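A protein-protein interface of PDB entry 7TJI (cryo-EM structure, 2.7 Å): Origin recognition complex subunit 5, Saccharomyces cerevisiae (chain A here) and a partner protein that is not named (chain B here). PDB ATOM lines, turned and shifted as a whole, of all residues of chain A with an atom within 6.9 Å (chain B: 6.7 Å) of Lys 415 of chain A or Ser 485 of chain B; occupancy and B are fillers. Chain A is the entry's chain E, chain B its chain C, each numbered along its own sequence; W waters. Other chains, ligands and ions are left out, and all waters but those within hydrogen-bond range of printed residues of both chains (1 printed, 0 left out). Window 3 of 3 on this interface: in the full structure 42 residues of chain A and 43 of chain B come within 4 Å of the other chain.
N of Ala 416 of chain A is in hydrogen-bond range of O of Ile 616 of chain B.
ND2 of Asn 486 of chain B lies close to O of Ser 482 of chain B (3.2 Å). The side-chain carboxylate (OE2) of Glu 488 of chain B lies within salt-bridge range of the side-chain amino group (NZ) of Lys 484 of chain B (2.6 Å). The chain-end carboxylate (OXT) of Ile 616 of chain B lies within salt-bridge range of the side-chain amino group (NZ) of Lys 484 of chain B (2.8 Å). The side-chain carboxylate (OE1) of Glu 488 of chain B sits at hydrogen-bond distance from the backbone NH (N) of Gly 615 of chain B, at 3.3 Å. The side-chain amide oxygen of Gln 391 of chain A sits close to the backbone carbonyl oxygen of Met 414 of chain A (3.2 Å).
Among the printed residues, pairs that only touch across the chains: Lys 415 of chain A with Ser 485 of chain B (3.4 Å), Lys 415 of chain A with Ile 616 of chain B (3.4 Å), Gln 391 of chain A with Ile 616 of chain B (3.6 Å), Ala 416 of chain A with Lys 484 of chain B (3.7 Å), Ile 418 of chain A with Tyr 483 of chain B (3.7 Å), Gln 391 of chain A with Gly 615 of chain B (3.7 Å) and Asn 417 of chain A with Ser 482 of chain B (3.8 Å).
Of the printed residues of chain B, Ala 416 of chain A touches Lys 484 and Ile 616. Printed residues of chain B within 4 Å of Ile 418 of chain A: Tyr 483. Of the printed residues of chain A, Ser 482 of chain B touches Asn 417 (3.8 Å). Of the printed residues of chain A, Lys 484 of chain B touches Ala 416. Of chain A, only Lys 415 (3.4 Å) comes within 4 Å of Ser 485 of chain B. Printed residues of chain A within 4 Å of Ile 616 of chain B: Gln 391, Lys 415 and Ala 416. The nearest residue of chain B that does not touch Lys 415 of chain A is Ser 482 of chain B (4.2 Å). The nearest printed residue of chain A that does not touch Ile 616 of chain B is Met 414 of chain A (4.6 Å).
Hydrophobic or aromatic side chains of chain B within 4 Å of the printed part of chain A: Tyr 483 and Ile 616. Of the 10 printed residues of chain A, 5 touch a printed residue of chain B. Hydrophobic or aromatic side chains of chain A within 4 Å of the printed part of chain B: Ala 416 and Ile 418. Among the printed residues, no Asp or Glu carboxylate lies within 4 Å of a Lys or Arg side-chain nitrogen of the other chain.
Water W1 bridges O of Ala 416 of chain A (2.7 Å) and N of Lys 484 of chain B (3.3 Å).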
ATOM      1  N   PHE A 390      22.922  21.106   8.420  1.00  0.00           N
ATOM      2  CA  PHE A 390      23.892  22.183   8.224  1.00  0.00           C
ATOM      3  C   PHE A 390      25.323  21.658   8.203  1.00  0.00           C
ATOM      4  O   PHE A 390      26.123  22.048   7.347  1.00  0.00           O
ATOM      5  CB  PHE A 390      23.723  23.240   9.323  1.00  0.00           C
ATOM      6  CG  PHE A 390      24.873  24.217   9.427  1.00  0.00           C
ATOM      7  CD1 PHE A 390      24.960  25.291   8.559  1.00  0.00           C
ATOM      8  CD2 PHE A 390      25.845  24.080  10.415  1.00  0.00           C
ATOM      9  CE1 PHE A 390      26.005  26.197   8.656  1.00  0.00           C
ATOM     10  CE2 PHE A 390      26.892  24.975  10.509  1.00  0.00           C
ATOM     11  CZ  PHE A 390      26.970  26.036   9.632  1.00  0.00           C
ATOM     12  N   GLN A 391      25.670  20.784   9.142  1.00  0.00           N
ATOM     13  CA  GLN A 391      27.019  20.236   9.122  1.00  0.00           C
ATOM     14  C   GLN A 391      27.166  19.087   8.134  1.00  0.00           C
ATOM     15  O   GLN A 391      28.298  18.699   7.832  1.00  0.00           O
ATOM     16  CB  GLN A 391      27.449  19.802  10.527  1.00  0.00           C
ATOM     17  CG  GLN A 391      26.916  18.466  10.985  1.00  0.00           C
ATOM     18  CD  GLN A 391      27.867  17.752  11.933  1.00  0.00           C
ATOM     19  OE1 GLN A 391      29.068  18.006  11.932  1.00  0.00           O
ATOM     20  NE2 GLN A 391      27.328  16.854  12.749  1.00  0.00           N
ATOM     21  N   GLU A 411      39.916  17.978  13.022  1.00  0.00           N
ATOM     22  CA  GLU A 411      38.495  18.246  13.291  1.00  0.00           C
ATOM     23  C   GLU A 411      37.741  18.598  12.003  1.00  0.00           C
ATOM     24  O   GLU A 411      37.338  19.740  11.773  1.00  0.00           O
ATOM     25  CB  GLU A 411      38.339  19.334  14.363  1.00  0.00           C
ATOM     26  CG  GLU A 411      37.146  19.138  15.283  1.00  0.00           C
ATOM     27  CD  GLU A 411      35.913  19.877  14.812  1.00  0.00           C
ATOM     28  OE1 GLU A 411      36.043  21.046  14.392  1.00  0.00           O
ATOM     29  OE2 GLU A 411      34.812  19.288  14.863  1.00  0.00           O
ATOM     30  N   LEU A 413      34.805  17.743  10.537  1.00  0.00           N
ATOM     31  CA  LEU A 413      33.451  18.270  10.578  1.00  0.00           C
ATOM     32  C   LEU A 413      33.420  19.583  11.357  1.00  0.00           C
ATOM     33  O   LEU A 413      34.376  19.954  12.042  1.00  0.00           O
ATOM     34  CB  LEU A 413      32.494  17.250  11.194  1.00  0.00           C
ATOM     35  CG  LEU A 413      31.775  16.368  10.173  1.00  0.00           C
ATOM     36  CD1 LEU A 413      30.903  15.333  10.865  1.00  0.00           C
ATOM     37  CD2 LEU A 413      30.956  17.223   9.215  1.00  0.00           C
ATOM     38  N   MET A 414      32.309  20.303  11.242  1.00  0.00           N
ATOM     39  CA  MET A 414      32.130  21.557  11.963  1.00  0.00           C
ATOM     40  C   MET A 414      31.107  21.378  13.074  1.00  0.00           C
ATOM     41  O   MET A 414      29.981  20.938  12.825  1.00  0.00           O
ATOM     42  CB  MET A 414      31.692  22.687  11.034  1.00  0.00           C
ATOM     43  CG  MET A 414      32.223  24.035  11.478  1.00  0.00           C
ATOM     44  SD  MET A 414      31.278  25.431  10.861  1.00  0.00           S
ATOM     45  CE  MET A 414      32.042  26.758  11.781  1.00  0.00           C
ATOM     46  N   LYS A 415      31.507  21.717  14.295  1.00  0.00           N
ATOM     47  CA  LYS A 415      30.598  21.719  15.428  1.00  0.00           C
ATOM     48  C   LYS A 415      29.779  23.002  15.445  1.00  0.00           C
ATOM     49  O   LYS A 415      30.164  24.018  14.862  1.00  0.00           O
ATOM     50  CB  LYS A 415      31.372  21.584  16.738  1.00  0.00           C
ATOM     51  CG  LYS A 415      32.288  20.377  16.799  1.00  0.00           C
ATOM     52  CD  LYS A 415      33.299  20.516  17.923  1.00  0.00           C
ATOM     53  CE  LYS A 415      34.033  19.213  18.169  1.00  0.00           C
ATOM     54  NZ  LYS A 415      34.892  19.282  19.381  1.00  0.00           N
ATOM     55  N   ALA A 416      28.635  22.948  16.124  1.00  0.00           N
ATOM     56  CA  ALA A 416      27.789  24.125  16.314  1.00  0.00           C
ATOM     57  C   ALA A 416      28.292  24.883  17.538  1.00  0.00           C
ATOM     58  O   ALA A 416      27.915  24.597  18.674  1.00  0.00           O
ATOM     59  CB  ALA A 416      26.328  23.724  16.465  1.00  0.00           C
ATOM     60  N   ASN A 417      29.160  25.861  17.298  1.00  0.00           N
ATOM     61  CA  ASN A 417      29.759  26.671  18.350  1.00  0.00           C
ATOM     62  C   ASN A 417      28.920  27.935  18.567  1.00  0.00           C
ATOM     63  O   ASN A 417      27.748  27.982  18.182  1.00  0.00           O
ATOM     64  CB  ASN A 417      31.232  26.944  18.015  1.00  0.00           C
ATOM     65  CG  ASN A 417      31.411  27.970  16.916  1.00  0.00           C
ATOM     66  OD1 ASN A 417      30.673  27.988  15.932  1.00  0.00           O
ATOM     67  ND2 ASN A 417      32.401  28.834  17.081  1.00  0.00           N
ATOM     68  N   ILE A 418      29.497  28.936  19.245  1.00  0.00           N
ATOM     69  CA  ILE A 418      28.830  30.209  19.530  1.00  0.00           C
ATOM     70  C   ILE A 418      28.410  30.909  18.242  1.00  0.00           C
ATOM     71  O   ILE A 418      27.322  31.496  18.163  1.00  0.00           O
ATOM     72  CB  ILE A 418      29.766  31.103  20.374  1.00  0.00           C
ATOM     73  CG1 ILE A 418      30.064  30.467  21.719  1.00  0.00           C
ATOM     74  CG2 ILE A 418      29.185  32.489  20.614  1.00  0.00           C
ATOM     75  CD1 ILE A 418      28.894  30.001  22.468  1.00  0.00           C
ATOM     76  N   VAL A 420      27.611  29.729  15.236  1.00  0.00           N
ATOM     77  CA  VAL A 420      26.473  29.114  14.552  1.00  0.00           C
ATOM     78  C   VAL A 420      25.159  29.541  15.197  1.00  0.00           C
ATOM     79  O   VAL A 420      24.203  29.923  14.508  1.00  0.00           O
ATOM     80  CB  VAL A 420      26.628  27.582  14.547  1.00  0.00           C
ATOM     81  CG1 VAL A 420      25.463  26.921  13.828  1.00  0.00           C
ATOM     82  CG2 VAL A 420      27.954  27.186  13.915  1.00  0.00           C
ATOM     83  N   SER B 482      33.258  26.022  21.483  1.00  0.00           N
ATOM     84  CA  SER B 482      32.281  25.013  21.091  1.00  0.00           C
ATOM     85  C   SER B 482      31.532  24.648  22.360  1.00  0.00           C
ATOM     86  O   SER B 482      31.891  23.711  23.062  1.00  0.00           O
ATOM     87  CB  SER B 482      32.962  23.808  20.455  1.00  0.00           C
ATOM     88  OG  SER B 482      34.162  23.482  21.129  1.00  0.00           O
ATOM     89  N   TYR B 483      30.479  25.420  22.643  1.00  0.00           N
ATOM     90  CA  TYR B 483      29.813  25.426  23.944  1.00  0.00           C
ATOM     91  C   TYR B 483      29.134  24.093  24.231  1.00  0.00           C
ATOM     92  O   TYR B 483      29.415  23.429  25.245  1.00  0.00           O
ATOM     93  CB  TYR B 483      28.807  26.588  23.948  1.00  0.00           C
ATOM     94  CG  TYR B 483      27.807  26.689  25.081  1.00  0.00           C
ATOM     95  CD1 TYR B 483      26.576  26.033  25.022  1.00  0.00           C
ATOM     96  CD2 TYR B 483      28.055  27.503  26.172  1.00  0.00           C
ATOM     97  CE1 TYR B 483      25.659  26.138  26.047  1.00  0.00           C
ATOM     98  CE2 TYR B 483      27.132  27.626  27.191  1.00  0.00           C
ATOM     99  CZ  TYR B 483      25.941  26.937  27.127  1.00  0.00           C
ATOM    100  OH  TYR B 483      25.023  27.054  28.145  1.00  0.00           O
ATOM    101  N   LYS B 484      28.233  23.687  23.335  1.00  0.00           N
ATOM    102  CA  LYS B 484      27.520  22.437  23.532  1.00  0.00           C
ATOM    103  C   LYS B 484      28.454  21.247  23.393  1.00  0.00           C
ATOM    104  O   LYS B 484      28.290  20.271  24.121  1.00  0.00           O
ATOM    105  CB  LYS B 484      26.324  22.347  22.578  1.00  0.00           C
ATOM    106  CG  LYS B 484      26.616  22.117  21.112  1.00  0.00           C
ATOM    107  CD  LYS B 484      25.346  22.264  20.297  1.00  0.00           C
ATOM    108  CE  LYS B 484      24.306  21.235  20.704  1.00  0.00           C
ATOM    109  NZ  LYS B 484      24.761  19.848  20.427  1.00  0.00           N
ATOM    110  N   SER B 485      29.483  21.353  22.545  1.00  0.00           N
ATOM    111  CA  SER B 485      30.462  20.277  22.411  1.00  0.00           C
ATOM    112  C   SER B 485      31.283  20.111  23.681  1.00  0.00           C
ATOM    113  O   SER B 485      31.623  18.989  24.054  1.00  0.00           O
ATOM    114  CB  SER B 485      31.375  20.535  21.215  1.00  0.00           C
ATOM    115  OG  SER B 485      30.665  20.419  19.997  1.00  0.00           O
ATOM    116  N   ASN B 486      31.589  21.214  24.367  1.00  0.00           N
ATOM    117  CA  ASN B 486      32.287  21.140  25.645  1.00  0.00           C
ATOM    118  C   ASN B 486      31.418  20.497  26.713  1.00  0.00           C
ATOM    119  O   ASN B 486      31.913  19.688  27.507  1.00  0.00           O
ATOM    120  CB  ASN B 486      32.723  22.534  26.091  1.00  0.00           C
ATOM    121  CG  ASN B 486      33.885  23.060  25.293  1.00  0.00           C
ATOM    122  OD1 ASN B 486      34.625  22.297  24.676  1.00  0.00           O
ATOM    123  ND2 ASN B 486      34.043  24.376  25.280  1.00  0.00           N
ATOM    124  N   ILE B 487      30.123  20.843  26.733  1.00  0.00           N
ATOM    125  CA  ILE B 487      29.174  20.217  27.661  1.00  0.00           C
ATOM    126  C   ILE B 487      29.121  18.704  27.444  1.00  0.00           C
ATOM    127  O   ILE B 487      29.264  17.909  28.386  1.00  0.00           O
ATOM    128  CB  ILE B 487      27.779  20.847  27.491  1.00  0.00           C
ATOM    129  CG1 ILE B 487      27.773  22.298  27.968  1.00  0.00           C
ATOM    130  CG2 ILE B 487      26.727  20.034  28.218  1.00  0.00           C
ATOM    131  CD1 ILE B 487      28.065  22.446  29.422  1.00  0.00           C
ATOM    132  N   GLU B 488      28.956  18.302  26.184  1.00  0.00           N
ATOM    133  CA  GLU B 488      28.925  16.903  25.760  1.00  0.00           C
ATOM    134  C   GLU B 488      30.225  16.162  26.067  1.00  0.00           C
ATOM    135  O   GLU B 488      30.189  15.027  26.557  1.00  0.00           O
ATOM    136  CB  GLU B 488      28.609  16.913  24.270  1.00  0.00           C
ATOM    137  CG  GLU B 488      27.184  17.368  23.993  1.00  0.00           C
ATOM    138  CD  GLU B 488      26.996  17.832  22.562  1.00  0.00           C
ATOM    139  OE1 GLU B 488      27.710  17.370  21.669  1.00  0.00           O
ATOM    140  OE2 GLU B 488      26.124  18.694  22.337  1.00  0.00           O
ATOM    141  N   ASP B 489      31.376  16.789  25.801  1.00  0.00           N
ATOM    142  CA  ASP B 489      32.662  16.152  26.049  1.00  0.00           C
ATOM    143  C   ASP B 489      32.915  15.972  27.536  1.00  0.00           C
ATOM    144  O   ASP B 489      33.429  14.925  27.950  1.00  0.00           O
ATOM    145  CB  ASP B 489      33.786  16.970  25.413  1.00  0.00           C
ATOM    146  CG  ASP B 489      33.956  16.680  23.931  1.00  0.00           C
ATOM    147  OD1 ASP B 489      33.163  15.887  23.383  1.00  0.00           O
ATOM    148  OD2 ASP B 489      34.886  17.242  23.318  1.00  0.00           O
ATOM    149  N   ASN B 490      32.546  16.967  28.354  1.00  0.00           N
ATOM    150  CA  ASN B 490      32.683  16.833  29.800  1.00  0.00           C
ATOM    151  C   ASN B 490      31.791  15.723  30.334  1.00  0.00           C
ATOM    152  O   ASN B 490      32.253  14.874  31.105  1.00  0.00           O
ATOM    153  CB  ASN B 490      32.355  18.157  30.493  1.00  0.00           C
ATOM    154  CG  ASN B 490      33.368  19.242  30.196  1.00  0.00           C
ATOM    155  OD1 ASN B 490      34.549  18.971  29.982  1.00  0.00           O
ATOM    156  ND2 ASN B 490      32.907  20.484  30.177  1.00  0.00           N
ATOM    157  N   ARG B 614      25.876  14.035  20.301  1.00  0.00           N
ATOM    158  CA  ARG B 614      27.239  14.509  20.460  1.00  0.00           C
ATOM    159  C   ARG B 614      27.889  14.720  19.093  1.00  0.00           C
ATOM    160  O   ARG B 614      27.499  14.115  18.093  1.00  0.00           O
ATOM    161  CB  ARG B 614      28.033  13.544  21.344  1.00  0.00           C
ATOM    162  CG  ARG B 614      29.365  14.052  21.850  1.00  0.00           C
ATOM    163  CD  ARG B 614      30.021  13.062  22.783  1.00  0.00           C
ATOM    164  NE  ARG B 614      31.420  13.396  23.018  1.00  0.00           N
ATOM    165  CZ  ARG B 614      32.419  13.029  22.226  1.00  0.00           C
ATOM    166  NH1 ARG B 614      32.210  12.305  21.140  1.00  0.00           N
ATOM    167  NH2 ARG B 614      33.659  13.400  22.531  1.00  0.00           N
ATOM    168  N   GLY B 615      28.830  15.658  19.037  1.00  0.00           N
ATOM    169  CA  GLY B 615      29.538  15.954  17.814  1.00  0.00           C
ATOM    170  C   GLY B 615      28.843  16.917  16.881  1.00  0.00           C
ATOM    171  O   GLY B 615      29.411  17.252  15.835  1.00  0.00           O
ATOM    172  N   ILE B 616      27.638  17.369  17.215  1.00  0.00           N
ATOM    173  CA  ILE B 616      26.962  18.376  16.411  1.00  0.00           C
ATOM    174  C   ILE B 616      26.983  19.721  17.135  1.00  0.00           C
ATOM    175  O   ILE B 616      27.717  20.637  16.763  1.00  0.00           O
ATOM    176  CB  ILE B 616      25.522  17.963  16.083  1.00  0.00           C
ATOM    177  CG1 ILE B 616      25.445  16.463  15.783  1.00  0.00           C
ATOM    178  CG2 ILE B 616      25.005  18.768  14.911  1.00  0.00           C
ATOM    179  CD1 ILE B 616      24.069  15.990  15.375  1.00  0.00           C
ATOM    180  OXT ILE B 616      26.267  19.919  18.116  1.00  0.00           O
HETATM  181  O   HOH W   1      27.319  25.852  21.008  1.00  0.00           O
